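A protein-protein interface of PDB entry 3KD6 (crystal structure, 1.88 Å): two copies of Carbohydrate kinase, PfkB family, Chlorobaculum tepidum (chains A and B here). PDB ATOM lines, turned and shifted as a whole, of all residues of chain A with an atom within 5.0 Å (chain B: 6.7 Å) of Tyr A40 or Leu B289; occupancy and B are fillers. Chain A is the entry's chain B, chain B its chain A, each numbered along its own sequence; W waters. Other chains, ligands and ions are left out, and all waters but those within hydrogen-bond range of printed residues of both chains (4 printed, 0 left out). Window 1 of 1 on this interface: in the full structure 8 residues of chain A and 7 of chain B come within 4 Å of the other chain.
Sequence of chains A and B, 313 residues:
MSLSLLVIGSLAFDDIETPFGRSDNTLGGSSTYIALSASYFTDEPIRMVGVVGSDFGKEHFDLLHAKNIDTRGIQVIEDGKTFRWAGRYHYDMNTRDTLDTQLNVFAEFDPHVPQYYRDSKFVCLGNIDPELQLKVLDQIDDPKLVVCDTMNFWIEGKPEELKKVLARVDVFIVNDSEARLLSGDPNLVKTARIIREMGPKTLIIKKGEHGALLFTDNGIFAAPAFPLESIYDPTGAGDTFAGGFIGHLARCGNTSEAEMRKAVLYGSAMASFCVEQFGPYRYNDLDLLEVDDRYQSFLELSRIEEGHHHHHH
The side-chain carboxylate of Asp B287 lies close to the side-chain carboxylate of Asp A292 (2.8 Å).
OD1 of Asp B287 sits at hydrogen-bond distance from N of Leu B289 (3.1 Å).
The backbone NH (N) of Glu B290 lies within hydrogen-bond range of the side-chain carboxylate (OD1) of Asp B287 (2.8 Å).
NZ of Lys A67 sits at hydrogen-bond distance from OH of Tyr A40, 3.3 Å away.
O of Tyr A283 sits at hydrogen-bond distance from OH of Tyr A40 (3.2 Å).
OH of Tyr A40 is in hydrogen-bond range of O of Leu A286, at 2.7 Å.
The side-chain carboxylate (OD1) of Asp A287 sits at hydrogen-bond distance from the backbone NH (N) of Leu A289 (3.1 Å).
Tyr A40 touches Leu B289.
CE1 of Tyr A266 touches CD1 of Leu B289, 3.8 Å away.
Leu A288 touches Leu B289.
CD1 of Leu A288 touches CB of Asp B292 (3.3 Å).
Leu A288 touches Asp B293 (CD1 to N, 3.4 Å).
Asp B293 touches Leu A289 (OD2 to CD1, 3.5 Å).
Val A291 touches Leu B289 (CG1 to CD1, 3.96 Å).
Asp A292 touches Leu B289.
Asp A292 touches Glu B290 (OD2 to CG, 3.8 Å).
Ser A37 touches none of the printed residues of chain B.
Of chain B, only Leu B289 (3.6 Å) comes within 4 Å of Tyr A40.
Lys A67 touches none of the printed residues of chain B.
Of the printed residues of chain B, Tyr A266 touches Leu B289 (3.8 Å).
Of the printed residues of chain B, Asp A292 touches Asp B287 (2.8 Å), Leu B289 (3.6 Å) and Glu B290 (3.8 Å).
Printed residues of chain A within 4 Å of Leu B289: Tyr A40 (3.6 Å), Tyr A266 (3.8 Å), Leu A288 (3.3 Å), Val A291 (3.96 Å) and Asp A292 (3.6 Å).
Printed residues of chain A within 4 Å of Asp B293: Leu A288 and Leu A289.
The nearest residue of chain A that does not touch Leu B289 is Phe A41 (4.4 Å).
Of the 17 printed residues of chain A, 6 touch a printed residue of chain B.
Printed residues of chain A that touch a printed residue of chain B: Tyr A40, Tyr A266, Leu A288, Leu A289, Val A291 and Asp A292.
Hydrophobic or aromatic side chains of chain A that line the printed part of chain B: Tyr A266, Leu A288, Leu A289 and Val A291.
Hydrophobic or aromatic side chains of chain B within 4 Å of the printed part of chain A: Leu B289.
Among the printed residues, no Asp or Glu carboxylate lies within 4 Å of a Lys or Arg side-chain nitrogen of the other chain.
Leu A288 touches Leu B289, but with the chains exchanged Leu A289 does not touch Leu B288 (7.7 Å).
Leu A288 touches Asp B292, but with the chains exchanged Asp A292 does not touch Leu B288 (6.7 Å).
Asp A292 touches Asp B287, but with the chains exchanged Asp A287 does not touch Asp B292 (8.7 Å).
Asp A292 touches Leu B289, but with the chains exchanged Leu A289 does not touch Asp B292 (7.2 Å).
Positions printed for both chains: 286, 287, 288, 289, 291 and 292.
Of the 10 pairs that touch across the chains among the printed residues, none has its exchanged pair printed and touching as well.
Water W4 lies within hydrogen-bond range of OH of Tyr A266 (2.5 Å), OD1 of Asp A292 (2.6 Å) and OD2 of Asp B287 (3.0 Å).
Water W3 lies within hydrogen-bond range of the side-chain carboxylate of Asp B292 and the backbone carbonyl oxygen of Tyr A40.
Water W2 lies within hydrogen-bond range of the backbone NH of Leu A288 and the side-chain carboxylate of Asp B293.
Water W1 lies within hydrogen-bond range of N of Leu B289 (3.1 Å), OH of Tyr A266 (3.2 Å), N of Leu B288 (3.4 Å) and OD1 of Asp B287 (3.4 Å).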
ATOM      1  N   LEU A  36      24.705 -13.572 -33.887  1.00  0.00           N
ATOM      2  CA  LEU A  36      25.707 -14.635 -33.841  1.00  0.00           C
ATOM      3  C   LEU A  36      25.677 -15.365 -32.493  1.00  0.00           C
ATOM      4  O   LEU A  36      25.782 -16.588 -32.439  1.00  0.00           O
ATOM      5  CB  LEU A  36      27.111 -14.071 -34.080  1.00  0.00           C
ATOM      6  CG  LEU A  36      27.422 -13.538 -35.485  1.00  0.00           C
ATOM      7  CD1 LEU A  36      28.811 -12.911 -35.497  1.00  0.00           C
ATOM      8  CD2 LEU A  36      27.314 -14.664 -36.507  1.00  0.00           C
ATOM      9  N   SER A  37      25.537 -14.606 -31.410  1.00  0.00           N
ATOM     10  CA  SER A  37      25.486 -15.195 -30.077  1.00  0.00           C
ATOM     11  C   SER A  37      24.218 -16.015 -29.876  1.00  0.00           C
ATOM     12  O   SER A  37      24.275 -17.144 -29.407  1.00  0.00           O
ATOM     13  CB  SER A  37      25.548 -14.107 -29.005  1.00  0.00           C
ATOM     14  OG  SER A  37      25.500 -14.689 -27.714  1.00  0.00           O
ATOM     15  N   ALA A  38      23.073 -15.444 -30.228  1.00  0.00           N
ATOM     16  CA  ALA A  38      21.796 -16.139 -30.065  1.00  0.00           C
ATOM     17  C   ALA A  38      21.689 -17.446 -30.864  1.00  0.00           C
ATOM     18  O   ALA A  38      20.999 -18.380 -30.440  1.00  0.00           O
ATOM     19  CB  ALA A  38      20.658 -15.211 -30.449  1.00  0.00           C
ATOM     20  N   SER A  39      22.354 -17.507 -32.018  1.00  0.00           N
ATOM     21  CA  SER A  39      22.315 -18.710 -32.862  1.00  0.00           C
ATOM     22  C   SER A  39      22.830 -19.954 -32.142  1.00  0.00           C
ATOM     23  O   SER A  39      22.489 -21.083 -32.518  1.00  0.00           O
ATOM     24  CB  SER A  39      23.125 -18.514 -34.153  1.00  0.00           C
ATOM     25  OG  SER A  39      24.517 -18.572 -33.903  1.00  0.00           O
ATOM     26  N   TYR A  40      23.655 -19.762 -31.117  1.00  0.00           N
ATOM     27  CA  TYR A  40      24.163 -20.899 -30.368  1.00  0.00           C
ATOM     28  C   TYR A  40      23.047 -21.579 -29.568  1.00  0.00           C
ATOM     29  O   TYR A  40      23.192 -22.725 -29.135  1.00  0.00           O
ATOM     30  CB  TYR A  40      25.280 -20.460 -29.410  1.00  0.00           C
ATOM     31  CG  TYR A  40      26.630 -20.359 -30.081  1.00  0.00           C
ATOM     32  CD1 TYR A  40      26.936 -19.291 -30.927  1.00  0.00           C
ATOM     33  CD2 TYR A  40      27.581 -21.367 -29.921  1.00  0.00           C
ATOM     34  CE1 TYR A  40      28.156 -19.232 -31.597  1.00  0.00           C
ATOM     35  CE2 TYR A  40      28.803 -21.323 -30.591  1.00  0.00           C
ATOM     36  CZ  TYR A  40      29.083 -20.252 -31.428  1.00  0.00           C
ATOM     37  OH  TYR A  40      30.288 -20.200 -32.098  1.00  0.00           O
ATOM     38  N   PHE A  41      21.927 -20.883 -29.408  1.00  0.00           N
ATOM     39  CA  PHE A  41      20.817 -21.391 -28.609  1.00  0.00           C
ATOM     40  C   PHE A  41      19.553 -21.803 -29.342  1.00  0.00           C
ATOM     41  O   PHE A  41      18.839 -22.699 -28.886  1.00  0.00           O
ATOM     42  CB  PHE A  41      20.469 -20.350 -27.545  1.00  0.00           C
ATOM     43  CG  PHE A  41      21.612 -20.040 -26.638  1.00  0.00           C
ATOM     44  CD1 PHE A  41      21.919 -20.885 -25.575  1.00  0.00           C
ATOM     45  CD2 PHE A  41      22.455 -18.968 -26.910  1.00  0.00           C
ATOM     46  CE1 PHE A  41      23.054 -20.672 -24.802  1.00  0.00           C
ATOM     47  CE2 PHE A  41      23.593 -18.745 -26.146  1.00  0.00           C
ATOM     48  CZ  PHE A  41      23.898 -19.597 -25.091  1.00  0.00           C
ATOM     49  N   THR A  42      19.268 -21.146 -30.460  1.00  0.00           N
ATOM     50  CA  THR A  42      18.069 -21.442 -31.241  1.00  0.00           C
ATOM     51  C   THR A  42      18.318 -22.582 -32.221  1.00  0.00           C
ATOM     52  O   THR A  42      19.448 -22.792 -32.661  1.00  0.00           O
ATOM     53  CB  THR A  42      17.619 -20.214 -32.043  1.00  0.00           C
ATOM     54  OG1 THR A  42      18.697 -19.777 -32.875  1.00  0.00           O
ATOM     55  CG2 THR A  42      17.216 -19.086 -31.115  1.00  0.00           C
ATOM     56  N   LYS A  67      25.777 -19.512 -39.715  1.00  0.00           N
ATOM     57  CA  LYS A  67      25.166 -19.737 -38.407  1.00  0.00           C
ATOM     58  C   LYS A  67      23.650 -19.887 -38.524  1.00  0.00           C
ATOM     59  O   LYS A  67      22.921 -19.728 -37.533  1.00  0.00           O
ATOM     60  CB  LYS A  67      25.484 -18.577 -37.456  1.00  0.00           C
ATOM     61  CG  LYS A  67      26.964 -18.369 -37.180  1.00  0.00           C
ATOM     62  CD  LYS A  67      27.544 -19.491 -36.344  1.00  0.00           C
ATOM     63  CE  LYS A  67      29.049 -19.313 -36.167  1.00  0.00           C
ATOM     64  NZ  LYS A  67      29.654 -20.404 -35.361  1.00  0.00           N
ATOM     65  N   TYR A 266      23.911 -17.676 -19.274  1.00  0.00           N
ATOM     66  CA  TYR A 266      24.280 -18.027 -20.642  1.00  0.00           C
ATOM     67  C   TYR A 266      24.796 -16.792 -21.377  1.00  0.00           C
ATOM     68  O   TYR A 266      25.734 -16.878 -22.174  1.00  0.00           O
ATOM     69  CB  TYR A 266      23.082 -18.598 -21.395  1.00  0.00           C
ATOM     70  CG  TYR A 266      22.813 -20.055 -21.095  1.00  0.00           C
ATOM     71  CD1 TYR A 266      23.754 -21.037 -21.418  1.00  0.00           C
ATOM     72  CD2 TYR A 266      21.613 -20.455 -20.511  1.00  0.00           C
ATOM     73  CE1 TYR A 266      23.502 -22.387 -21.169  1.00  0.00           C
ATOM     74  CE2 TYR A 266      21.352 -21.805 -20.257  1.00  0.00           C
ATOM     75  CZ  TYR A 266      22.300 -22.762 -20.589  1.00  0.00           C
ATOM     76  OH  TYR A 266      22.051 -24.094 -20.340  1.00  0.00           O
ATOM     77  N   MET A 270      28.549 -16.237 -23.161  1.00  0.00           N
ATOM     78  CA  MET A 270      28.806 -15.765 -24.520  1.00  0.00           C
ATOM     79  C   MET A 270      29.669 -14.506 -24.533  1.00  0.00           C
ATOM     80  O   MET A 270      30.596 -14.382 -25.336  1.00  0.00           O
ATOM     81  CB  MET A 270      27.487 -15.500 -25.253  1.00  0.00           C
ATOM     82  CG  MET A 270      26.616 -16.762 -25.437  1.00  0.00           C
ATOM     83  SD  MET A 270      27.548 -18.249 -26.234  1.00  0.00           S
ATOM     84  CE  MET A 270      27.902 -17.478 -27.959  1.00  0.00           C
ATOM     85  N   TYR A 283      33.863 -16.490 -32.476  1.00  0.00           N
ATOM     86  CA  TYR A 283      32.764 -17.399 -32.809  1.00  0.00           C
ATOM     87  C   TYR A 283      32.996 -18.245 -34.062  1.00  0.00           C
ATOM     88  O   TYR A 283      32.156 -19.067 -34.423  1.00  0.00           O
ATOM     89  CB  TYR A 283      31.448 -16.623 -32.948  1.00  0.00           C
ATOM     90  CG  TYR A 283      30.988 -15.983 -31.653  1.00  0.00           C
ATOM     91  CD1 TYR A 283      31.530 -16.371 -30.426  1.00  0.00           C
ATOM     92  CD2 TYR A 283      30.000 -15.001 -31.651  1.00  0.00           C
ATOM     93  CE1 TYR A 283      31.098 -15.796 -29.227  1.00  0.00           C
ATOM     94  CE2 TYR A 283      29.560 -14.420 -30.461  1.00  0.00           C
ATOM     95  CZ  TYR A 283      30.114 -14.823 -29.253  1.00  0.00           C
ATOM     96  OH  TYR A 283      29.685 -14.244 -28.083  1.00  0.00           O
ATOM     97  N   LEU A 286      34.283 -21.370 -31.976  1.00  0.00           N
ATOM     98  CA  LEU A 286      33.603 -21.690 -30.722  1.00  0.00           C
ATOM     99  C   LEU A 286      32.521 -22.745 -30.916  1.00  0.00           C
ATOM    100  O   LEU A 286      31.625 -22.574 -31.739  1.00  0.00           O
ATOM    101  CB  LEU A 286      32.974 -20.422 -30.123  1.00  0.00           C
ATOM    102  CG  LEU A 286      32.295 -20.563 -28.754  1.00  0.00           C
ATOM    103  CD1 LEU A 286      33.341 -20.853 -27.687  1.00  0.00           C
ATOM    104  CD2 LEU A 286      31.541 -19.279 -28.417  1.00  0.00           C
ATOM    105  N   ASP A 287      32.604 -23.837 -30.163  1.00  0.00           N
ATOM    106  CA  ASP A 287      31.602 -24.894 -30.275  1.00  0.00           C
ATOM    107  C   ASP A 287      30.718 -24.945 -29.031  1.00  0.00           C
ATOM    108  O   ASP A 287      31.095 -24.461 -27.969  1.00  0.00           O
ATOM    109  CB  ASP A 287      32.259 -26.259 -30.526  1.00  0.00           C
ATOM    110  CG  ASP A 287      33.120 -26.723 -29.372  1.00  0.00           C
ATOM    111  OD1 ASP A 287      32.616 -26.771 -28.232  1.00  0.00           O
ATOM    112  OD2 ASP A 287      34.299 -27.062 -29.605  1.00  0.00           O
ATOM    113  N   LEU A 288      29.544 -25.545 -29.177  1.00  0.00           N
ATOM    114  CA  LEU A 288      28.565 -25.636 -28.100  1.00  0.00           C
ATOM    115  C   LEU A 288      29.032 -26.191 -26.758  1.00  0.00           C
ATOM    116  O   LEU A 288      28.546 -25.758 -25.713  1.00  0.00           O
ATOM    117  CB  LEU A 288      27.354 -26.440 -28.577  1.00  0.00           C
ATOM    118  CG  LEU A 288      26.597 -25.849 -29.766  1.00  0.00           C
ATOM    119  CD1 LEU A 288      25.566 -26.843 -30.254  1.00  0.00           C
ATOM    120  CD2 LEU A 288      25.932 -24.547 -29.362  1.00  0.00           C
ATOM    121  N   LEU A 289      29.950 -27.154 -26.770  1.00  0.00           N
ATOM    122  CA  LEU A 289      30.424 -27.735 -25.518  1.00  0.00           C
ATOM    123  C   LEU A 289      31.297 -26.746 -24.745  1.00  0.00           C
ATOM    124  O   LEU A 289      31.310 -26.759 -23.516  1.00  0.00           O
ATOM    125  CB  LEU A 289      31.180 -29.042 -25.784  1.00  0.00           C
ATOM    126  CG  LEU A 289      30.388 -30.124 -26.533  1.00  0.00           C
ATOM    127  CD1 LEU A 289      31.175 -31.426 -26.511  1.00  0.00           C
ATOM    128  CD2 LEU A 289      29.018 -30.330 -25.882  1.00  0.00           C
ATOM    129  N   VAL A 291      30.818 -23.561 -24.775  1.00  0.00           N
ATOM    130  CA  VAL A 291      29.815 -22.657 -24.229  1.00  0.00           C
ATOM    131  C   VAL A 291      29.158 -23.267 -22.990  1.00  0.00           C
ATOM    132  O   VAL A 291      28.984 -22.591 -21.978  1.00  0.00           O
ATOM    133  CB  VAL A 291      28.723 -22.345 -25.270  1.00  0.00           C
ATOM    134  CG1 VAL A 291      27.584 -21.573 -24.620  1.00  0.00           C
ATOM    135  CG2 VAL A 291      29.324 -21.546 -26.428  1.00  0.00           C
ATOM    136  N   ASP A 292      28.816 -24.553 -23.070  1.00  0.00           N
ATOM    137  CA  ASP A 292      28.179 -25.244 -21.953  1.00  0.00           C
ATOM    138  C   ASP A 292      29.132 -25.258 -20.749  1.00  0.00           C
ATOM    139  O   ASP A 292      28.716 -24.998 -19.623  1.00  0.00           O
ATOM    140  CB  ASP A 292      27.785 -26.671 -22.378  1.00  0.00           C
ATOM    141  CG  ASP A 292      26.737 -27.301 -21.458  1.00  0.00           C
ATOM    142  OD1 ASP A 292      25.819 -26.588 -21.009  1.00  0.00           O
ATOM    143  OD2 ASP A 292      26.817 -28.521 -21.197  1.00  0.00           O
ATOM    144  N   LEU B 286      21.235 -34.165 -19.141  1.00  0.00           N
ATOM    145  CA  LEU B 286      21.500 -33.866 -20.557  1.00  0.00           C
ATOM    146  C   LEU B 286      20.837 -32.532 -20.926  1.00  0.00           C
ATOM    147  O   LEU B 286      19.646 -32.347 -20.682  1.00  0.00           O
ATOM    148  CB  LEU B 286      20.927 -34.977 -21.448  1.00  0.00           C
ATOM    149  CG  LEU B 286      21.071 -34.811 -22.970  1.00  0.00           C
ATOM    150  CD1 LEU B 286      22.548 -34.881 -23.357  1.00  0.00           C
ATOM    151  CD2 LEU B 286      20.282 -35.893 -23.691  1.00  0.00           C
ATOM    152  N   ASP B 287      21.598 -31.610 -21.517  1.00  0.00           N
ATOM    153  CA  ASP B 287      21.036 -30.309 -21.889  1.00  0.00           C
ATOM    154  C   ASP B 287      21.006 -30.080 -23.397  1.00  0.00           C
ATOM    155  O   ASP B 287      21.667 -30.779 -24.154  1.00  0.00           O
ATOM    156  CB  ASP B 287      21.810 -29.170 -21.204  1.00  0.00           C
ATOM    157  CG  ASP B 287      23.278 -29.151 -21.580  1.00  0.00           C
ATOM    158  OD1 ASP B 287      23.583 -29.106 -22.790  1.00  0.00           O
ATOM    159  OD2 ASP B 287      24.129 -29.173 -20.664  1.00  0.00           O
ATOM    160  N   LEU B 288      20.241 -29.079 -23.817  1.00  0.00           N
ATOM    161  CA  LEU B 288      20.083 -28.753 -25.229  1.00  0.00           C
ATOM    162  C   LEU B 288      21.388 -28.454 -25.972  1.00  0.00           C
ATOM    163  O   LEU B 288      21.531 -28.807 -27.139  1.00  0.00           O
ATOM    164  CB  LEU B 288      19.116 -27.580 -25.376  1.00  0.00           C
ATOM    165  CG  LEU B 288      17.693 -27.891 -24.907  1.00  0.00           C
ATOM    166  CD1 LEU B 288      16.894 -26.604 -24.767  1.00  0.00           C
ATOM    167  CD2 LEU B 288      17.029 -28.843 -25.888  1.00  0.00           C
ATOM    168  N   LEU B 289      22.335 -27.796 -25.315  1.00  0.00           N
ATOM    169  CA  LEU B 289      23.600 -27.509 -25.971  1.00  0.00           C
ATOM    170  C   LEU B 289      24.271 -28.825 -26.367  1.00  0.00           C
ATOM    171  O   LEU B 289      24.849 -28.940 -27.447  1.00  0.00           O
ATOM    172  CB  LEU B 289      24.516 -26.702 -25.041  1.00  0.00           C
ATOM    173  CG  LEU B 289      24.241 -25.195 -24.967  1.00  0.00           C
ATOM    174  CD1 LEU B 289      25.089 -24.552 -23.872  1.00  0.00           C
ATOM    175  CD2 LEU B 289      24.558 -24.557 -26.322  1.00  0.00           C
ATOM    176  N   GLU B 290      24.190 -29.813 -25.478  1.00  0.00           N
ATOM    177  CA  GLU B 290      24.782 -31.122 -25.721  1.00  0.00           C
ATOM    178  C   GLU B 290      24.065 -31.851 -26.850  1.00  0.00           C
ATOM    179  O   GLU B 290      24.700 -32.513 -27.678  1.00  0.00           O
ATOM    180  CB  GLU B 290      24.717 -31.962 -24.452  1.00  0.00           C
ATOM    181  CG  GLU B 290      25.596 -31.453 -23.318  1.00  0.00           C
ATOM    182  CD  GLU B 290      25.463 -32.314 -22.080  1.00  0.00           C
ATOM    183  OE1 GLU B 290      24.365 -32.308 -21.487  1.00  0.00           O
ATOM    184  OE2 GLU B 290      26.443 -32.999 -21.710  1.00  0.00           O
ATOM    185  N   VAL B 291      22.740 -31.752 -26.863  1.00  0.00           N
ATOM    186  CA  VAL B 291      21.950 -32.393 -27.915  1.00  0.00           C
ATOM    187  C   VAL B 291      22.264 -31.748 -29.270  1.00  0.00           C
ATOM    188  O   VAL B 291      22.490 -32.443 -30.269  1.00  0.00           O
ATOM    189  CB  VAL B 291      20.448 -32.270 -27.630  1.00  0.00           C
ATOM    190  CG1 VAL B 291      19.646 -32.677 -28.859  1.00  0.00           C
ATOM    191  CG2 VAL B 291      20.084 -33.141 -26.426  1.00  0.00           C
ATOM    192  N   ASP B 292      22.283 -30.417 -29.304  1.00  0.00           N
ATOM    193  CA  ASP B 292      22.588 -29.708 -30.543  1.00  0.00           C
ATOM    194  C   ASP B 292      23.973 -30.080 -31.050  1.00  0.00           C
ATOM    195  O   ASP B 292      24.187 -30.234 -32.249  1.00  0.00           O
ATOM    196  CB  ASP B 292      22.534 -28.190 -30.337  1.00  0.00           C
ATOM    197  CG  ASP B 292      21.117 -27.657 -30.268  1.00  0.00           C
ATOM    198  OD1 ASP B 292      20.175 -28.406 -30.593  1.00  0.00           O
ATOM    199  OD2 ASP B 292      20.944 -26.478 -29.899  1.00  0.00           O
ATOM    200  N   ASP B 293      24.918 -30.214 -30.128  1.00  0.00           N
ATOM    201  CA  ASP B 293      26.277 -30.565 -30.506  1.00  0.00           C
ATOM    202  C   ASP B 293      26.355 -31.967 -31.110  1.00  0.00           C
ATOM    203  O   ASP B 293      27.075 -32.193 -32.081  1.00  0.00           O
ATOM    204  CB  ASP B 293      27.199 -30.499 -29.292  1.00  0.00           C
ATOM    205  CG  ASP B 293      28.617 -30.888 -29.628  1.00  0.00           C
ATOM    206  OD1 ASP B 293      29.315 -30.068 -30.264  1.00  0.00           O
ATOM    207  OD2 ASP B 293      29.026 -32.015 -29.273  1.00  0.00           O
ATOM    208  N   ARG B 294      25.616 -32.909 -30.532  1.00  0.00           N
ATOM    209  CA  ARG B 294      25.643 -34.288 -31.017  1.00  0.00           C
ATOM    210  C   ARG B 294      24.973 -34.400 -32.387  1.00  0.00           C
ATOM    211  O   ARG B 294      25.399 -35.185 -33.240  1.00  0.00           O
ATOM    212  CB  ARG B 294      24.970 -35.217 -29.997  1.00  0.00           C
ATOM    213  CG  ARG B 294      25.064 -36.706 -30.335  1.00  0.00           C
ATOM    214  CD  ARG B 294      26.503 -37.163 -30.580  1.00  0.00           C
ATOM    215  NE  ARG B 294      27.391 -36.904 -29.446  1.00  0.00           N
ATOM    216  CZ  ARG B 294      27.415 -37.603 -28.312  1.00  0.00           C
ATOM    217  NH1 ARG B 294      26.595 -38.631 -28.126  1.00  0.00           N
ATOM    218  NH2 ARG B 294      28.277 -37.276 -27.359  1.00  0.00           N
HETATM  219  O   HOH W   1      21.729 -26.206 -22.706  1.00  0.00           O
HETATM  220  O   HOH W   2      29.280 -27.306 -31.291  1.00  0.00           O
HETATM  221  O   HOH W   3      22.123 -25.058 -27.875  1.00  0.00           O
HETATM  222  O   HOH W   4      23.321 -26.292 -20.542  1.00  0.00           O
